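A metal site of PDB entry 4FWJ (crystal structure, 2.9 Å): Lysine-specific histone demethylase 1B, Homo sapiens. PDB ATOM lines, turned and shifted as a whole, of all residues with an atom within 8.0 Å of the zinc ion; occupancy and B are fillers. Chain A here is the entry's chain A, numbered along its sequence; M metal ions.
The zinc ion is bound by NE2 of His 64, ND1 of His 58, SG of Cys 27 and SG of Cys 32.
Residues that only touch the zinc ion: Ser 60.
Five residues have an atom within 4 Å of the zinc ion: Cys 27, Cys 32, His 58, Ser 60 and His 64.
The nearest printed residue that does not touch the zinc ion is Lys 29 (4.8 Å).
N of His 58 is in hydrogen-bond range of OE1 of Glu 28 (3.0 Å).
The backbone carbonyl oxygen of Met 178 sits at hydrogen-bond distance from a ring nitrogen (NE2) of His 58 (2.7 Å).
The backbone NH of Lys 29 sits close to the side-chain sulfur of Cys 27, 3.4 Å away.
The side-chain sulfur (SG) of Cys 32 lies close to the backbone NH (N) of Ala 34 (3.5 Å).
The side-chain hydroxyl (OG) of Ser 60 is in hydrogen-bond range of the side-chain carboxylate (OE1) of Glu 63 (2.7 Å).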
ATOM      1  N   LYS A  26      13.110  12.222  -1.757  1.00  0.00           N
ATOM      2  CA  LYS A  26      13.090  12.080  -0.302  1.00  0.00           C
ATOM      3  C   LYS A  26      12.460  13.314   0.372  1.00  0.00           C
ATOM      4  O   LYS A  26      12.557  14.424  -0.134  1.00  0.00           O
ATOM      5  CB  LYS A  26      14.485  11.753   0.256  1.00  0.00           C
ATOM      6  CG  LYS A  26      15.543  12.837   0.019  1.00  0.00           C
ATOM      7  CD  LYS A  26      15.978  13.511   1.323  1.00  0.00           C
ATOM      8  CE  LYS A  26      16.187  15.013   1.176  1.00  0.00           C
ATOM      9  NZ  LYS A  26      16.993  15.429  -0.007  1.00  0.00           N
ATOM     10  N   CYS A  27      11.793  13.080   1.510  1.00  0.00           N
ATOM     11  CA  CYS A  27      11.136  14.125   2.279  1.00  0.00           C
ATOM     12  C   CYS A  27      12.065  15.297   2.687  1.00  0.00           C
ATOM     13  O   CYS A  27      13.300  15.166   2.673  1.00  0.00           O
ATOM     14  CB  CYS A  27      10.496  13.470   3.507  1.00  0.00           C
ATOM     15  SG  CYS A  27       9.833  14.576   4.767  1.00  0.00           S
ATOM     16  N   GLU A  28      11.475  16.448   3.037  1.00  0.00           N
ATOM     17  CA  GLU A  28      12.248  17.638   3.441  1.00  0.00           C
ATOM     18  C   GLU A  28      12.877  17.533   4.832  1.00  0.00           C
ATOM     19  O   GLU A  28      13.885  18.186   5.098  1.00  0.00           O
ATOM     20  CB  GLU A  28      11.380  18.910   3.356  1.00  0.00           C
ATOM     21  CG  GLU A  28      10.229  18.938   4.345  1.00  0.00           C
ATOM     22  CD  GLU A  28       9.490  20.277   4.385  1.00  0.00           C
ATOM     23  OE1 GLU A  28       8.311  20.272   4.805  1.00  0.00           O
ATOM     24  OE2 GLU A  28      10.081  21.314   4.008  1.00  0.00           O
ATOM     25  N   LYS A  29      12.280  16.722   5.709  1.00  0.00           N
ATOM     26  CA  LYS A  29      12.660  16.624   7.127  1.00  0.00           C
ATOM     27  C   LYS A  29      13.646  15.482   7.384  1.00  0.00           C
ATOM     28  O   LYS A  29      13.396  14.342   7.017  1.00  0.00           O
ATOM     29  CB  LYS A  29      11.404  16.488   7.995  1.00  0.00           C
ATOM     30  CG  LYS A  29      11.597  15.969   9.431  1.00  0.00           C
ATOM     31  CD  LYS A  29      11.761  17.085  10.453  1.00  0.00           C
ATOM     32  CE  LYS A  29      13.217  17.465  10.746  1.00  0.00           C
ATOM     33  NZ  LYS A  29      13.746  16.839  11.992  1.00  0.00           N
ATOM     34  N   ALA A  30      14.752  15.817   8.046  1.00  0.00           N
ATOM     35  CA  ALA A  30      15.779  14.847   8.442  1.00  0.00           C
ATOM     36  C   ALA A  30      15.211  13.711   9.302  1.00  0.00           C
ATOM     37  O   ALA A  30      14.419  13.948  10.222  1.00  0.00           O
ATOM     38  CB  ALA A  30      16.905  15.559   9.184  1.00  0.00           C
ATOM     39  N   GLY A  31      15.603  12.487   8.991  1.00  0.00           N
ATOM     40  CA  GLY A  31      15.178  11.332   9.776  1.00  0.00           C
ATOM     41  C   GLY A  31      13.735  10.883   9.586  1.00  0.00           C
ATOM     42  O   GLY A  31      13.297   9.961  10.278  1.00  0.00           O
ATOM     43  N   CYS A  32      13.006  11.511   8.664  1.00  0.00           N
ATOM     44  CA  CYS A  32      11.638  11.076   8.371  1.00  0.00           C
ATOM     45  C   CYS A  32      11.605   9.629   7.866  1.00  0.00           C
ATOM     46  O   CYS A  32      12.389   9.250   6.985  1.00  0.00           O
ATOM     47  CB  CYS A  32      10.961  12.001   7.350  1.00  0.00           C
ATOM     48  SG  CYS A  32       9.406  11.322   6.691  1.00  0.00           S
ATOM     49  N   THR A  33      10.681   8.850   8.435  1.00  0.00           N
ATOM     50  CA  THR A  33      10.613   7.398   8.223  1.00  0.00           C
ATOM     51  C   THR A  33      10.004   6.943   6.881  1.00  0.00           C
ATOM     52  O   THR A  33      10.115   5.772   6.550  1.00  0.00           O
ATOM     53  CB  THR A  33       9.867   6.662   9.370  1.00  0.00           C
ATOM     54  OG1 THR A  33       8.474   7.020   9.366  1.00  0.00           O
ATOM     55  CG2 THR A  33      10.484   7.007  10.726  1.00  0.00           C
ATOM     56  N   ALA A  34       9.355   7.842   6.143  1.00  0.00           N
ATOM     57  CA  ALA A  34       8.782   7.492   4.838  1.00  0.00           C
ATOM     58  C   ALA A  34       9.876   7.344   3.776  1.00  0.00           C
ATOM     59  O   ALA A  34      10.483   8.325   3.355  1.00  0.00           O
ATOM     60  CB  ALA A  34       7.744   8.519   4.392  1.00  0.00           C
ATOM     61  N   THR A  35      10.108   6.099   3.351  1.00  0.00           N
ATOM     62  CA  THR A  35      11.079   5.787   2.303  1.00  0.00           C
ATOM     63  C   THR A  35      10.608   6.371   0.980  1.00  0.00           C
ATOM     64  O   THR A  35      11.392   6.959   0.242  1.00  0.00           O
ATOM     65  CB  THR A  35      11.231   4.268   2.093  1.00  0.00           C
ATOM     66  OG1 THR A  35      10.775   3.572   3.266  1.00  0.00           O
ATOM     67  CG2 THR A  35      12.671   3.899   1.779  1.00  0.00           C
ATOM     68  N   PRO A  37       7.857   8.874  -0.272  1.00  0.00           N
ATOM     69  CA  PRO A  37       6.781   9.832  -0.092  1.00  0.00           C
ATOM     70  C   PRO A  37       5.876   9.835  -1.310  1.00  0.00           C
ATOM     71  O   PRO A  37       6.343   9.750  -2.445  1.00  0.00           O
ATOM     72  CB  PRO A  37       7.507  11.176   0.042  1.00  0.00           C
ATOM     73  CG  PRO A  37       8.926  10.846   0.319  1.00  0.00           C
ATOM     74  CD  PRO A  37       9.171   9.543  -0.373  1.00  0.00           C
ATOM     75  N   TRP A  56       9.394  18.071  -1.107  1.00  0.00           N
ATOM     76  CA  TRP A  56       8.320  17.302  -0.465  1.00  0.00           C
ATOM     77  C   TRP A  56       8.003  17.881   0.889  1.00  0.00           C
ATOM     78  O   TRP A  56       8.763  17.723   1.841  1.00  0.00           O
ATOM     79  CB  TRP A  56       8.744  15.851  -0.263  1.00  0.00           C
ATOM     80  CG  TRP A  56       8.522  14.921  -1.420  1.00  0.00           C
ATOM     81  CD1 TRP A  56       9.484  14.158  -2.085  1.00  0.00           C
ATOM     82  CD2 TRP A  56       7.253  14.568  -2.063  1.00  0.00           C
ATOM     83  NE1 TRP A  56       8.909  13.403  -3.081  1.00  0.00           N
ATOM     84  CE2 TRP A  56       7.581  13.604  -3.127  1.00  0.00           C
ATOM     85  CE3 TRP A  56       5.930  14.952  -1.892  1.00  0.00           C
ATOM     86  CZ2 TRP A  56       6.610  13.058  -3.954  1.00  0.00           C
ATOM     87  CZ3 TRP A  56       4.957  14.397  -2.734  1.00  0.00           C
ATOM     88  CH2 TRP A  56       5.296  13.479  -3.745  1.00  0.00           C
ATOM     89  N   TYR A  57       6.862  18.559   0.994  1.00  0.00           N
ATOM     90  CA  TYR A  57       6.416  19.072   2.282  1.00  0.00           C
ATOM     91  C   TYR A  57       5.909  17.965   3.203  1.00  0.00           C
ATOM     92  O   TYR A  57       5.190  17.058   2.775  1.00  0.00           O
ATOM     93  CB  TYR A  57       5.362  20.156   2.058  1.00  0.00           C
ATOM     94  CG  TYR A  57       5.911  21.320   1.265  1.00  0.00           C
ATOM     95  CD1 TYR A  57       6.381  22.467   1.905  1.00  0.00           C
ATOM     96  CD2 TYR A  57       5.987  21.266  -0.129  1.00  0.00           C
ATOM     97  CE1 TYR A  57       6.899  23.535   1.196  1.00  0.00           C
ATOM     98  CE2 TYR A  57       6.503  22.326  -0.854  1.00  0.00           C
ATOM     99  CZ  TYR A  57       6.953  23.459  -0.190  1.00  0.00           C
ATOM    100  OH  TYR A  57       7.469  24.519  -0.914  1.00  0.00           O
ATOM    101  N   HIS A  58       6.322  18.026   4.464  1.00  0.00           N
ATOM    102  CA  HIS A  58       6.054  16.989   5.469  1.00  0.00           C
ATOM    103  C   HIS A  58       4.969  17.461   6.404  1.00  0.00           C
ATOM    104  O   HIS A  58       5.088  18.540   7.014  1.00  0.00           O
ATOM    105  CB  HIS A  58       7.360  16.694   6.206  1.00  0.00           C
ATOM    106  CG  HIS A  58       7.232  15.823   7.440  1.00  0.00           C
ATOM    107  ND1 HIS A  58       7.839  14.621   7.541  1.00  0.00           N
ATOM    108  CD2 HIS A  58       6.613  16.047   8.665  1.00  0.00           C
ATOM    109  CE1 HIS A  58       7.593  14.089   8.750  1.00  0.00           C
ATOM    110  NE2 HIS A  58       6.846  14.949   9.440  1.00  0.00           N
ATOM    111  N   LEU A  59       3.890  16.700   6.512  1.00  0.00           N
ATOM    112  CA  LEU A  59       2.875  16.932   7.550  1.00  0.00           C
ATOM    113  C   LEU A  59       3.087  15.978   8.720  1.00  0.00           C
ATOM    114  O   LEU A  59       3.031  16.382   9.878  1.00  0.00           O
ATOM    115  CB  LEU A  59       1.462  16.770   7.019  1.00  0.00           C
ATOM    116  CG  LEU A  59       0.877  17.909   6.174  1.00  0.00           C
ATOM    117  CD1 LEU A  59      -0.560  17.555   5.805  1.00  0.00           C
ATOM    118  CD2 LEU A  59       0.917  19.261   6.876  1.00  0.00           C
ATOM    119  N   SER A  60       3.299  14.715   8.401  1.00  0.00           N
ATOM    120  CA  SER A  60       3.621  13.689   9.377  1.00  0.00           C
ATOM    121  C   SER A  60       4.485  12.653   8.662  1.00  0.00           C
ATOM    122  O   SER A  60       4.827  12.825   7.488  1.00  0.00           O
ATOM    123  CB  SER A  60       2.347  13.033   9.903  1.00  0.00           C
ATOM    124  OG  SER A  60       1.676  12.350   8.861  1.00  0.00           O
ATOM    125  N   CYS A  61       4.834  11.584   9.360  1.00  0.00           N
ATOM    126  CA  CYS A  61       5.628  10.514   8.773  1.00  0.00           C
ATOM    127  C   CYS A  61       4.941   9.817   7.601  1.00  0.00           C
ATOM    128  O   CYS A  61       5.602   9.419   6.640  1.00  0.00           O
ATOM    129  CB  CYS A  61       6.042   9.524   9.850  1.00  0.00           C
ATOM    130  SG  CYS A  61       7.497  10.119  10.741  1.00  0.00           S
ATOM    131  N   GLY A  62       3.622   9.683   7.659  1.00  0.00           N
ATOM    132  CA  GLY A  62       2.907   9.027   6.588  1.00  0.00           C
ATOM    133  C   GLY A  62       2.259   9.987   5.597  1.00  0.00           C
ATOM    134  O   GLY A  62       1.640   9.543   4.628  1.00  0.00           O
ATOM    135  N   GLU A  63       2.380  11.289   5.845  1.00  0.00           N
ATOM    136  CA  GLU A  63       1.628  12.267   5.044  1.00  0.00           C
ATOM    137  C   GLU A  63       2.466  13.378   4.421  1.00  0.00           C
ATOM    138  O   GLU A  63       3.041  14.201   5.134  1.00  0.00           O
ATOM    139  CB  GLU A  63       0.453  12.821   5.852  1.00  0.00           C
ATOM    140  CG  GLU A  63      -0.714  11.847   5.890  1.00  0.00           C
ATOM    141  CD  GLU A  63      -1.489  11.869   7.192  1.00  0.00           C
ATOM    142  OE1 GLU A  63      -0.962  12.345   8.236  1.00  0.00           O
ATOM    143  OE2 GLU A  63      -2.628  11.371   7.170  1.00  0.00           O
ATOM    144  N   HIS A  64       2.520  13.393   3.092  1.00  0.00           N
ATOM    145  CA  HIS A  64       3.340  14.352   2.344  1.00  0.00           C
ATOM    146  C   HIS A  64       2.597  14.902   1.155  1.00  0.00           C
ATOM    147  O   HIS A  64       1.732  14.234   0.593  1.00  0.00           O
ATOM    148  CB  HIS A  64       4.625  13.678   1.847  1.00  0.00           C
ATOM    149  CG  HIS A  64       5.476  13.124   2.959  1.00  0.00           C
ATOM    150  ND1 HIS A  64       5.202  11.953   3.561  1.00  0.00           N
ATOM    151  CD2 HIS A  64       6.625  13.627   3.568  1.00  0.00           C
ATOM    152  CE1 HIS A  64       6.124  11.719   4.520  1.00  0.00           C
ATOM    153  NE2 HIS A  64       6.991  12.737   4.523  1.00  0.00           N
ATOM    154  N   MET A 178       6.938  13.713  15.254  1.00  0.00           N
ATOM    155  CA  MET A 178       7.197  14.103  13.877  1.00  0.00           C
ATOM    156  C   MET A 178       5.991  14.756  13.194  1.00  0.00           C
ATOM    157  O   MET A 178       6.003  15.021  11.991  1.00  0.00           O
ATOM    158  CB  MET A 178       7.680  12.889  13.091  1.00  0.00           C
ATOM    159  CG  MET A 178       8.871  12.207  13.718  1.00  0.00           C
ATOM    160  SD  MET A 178      10.353  12.252  12.685  1.00  0.00           S
ATOM    161  CE  MET A 178      10.539  14.012  12.427  1.00  0.00           C
HETATM  162 ZN    ZN M   1       8.417  13.293   5.923  1.00  0.00          ZN
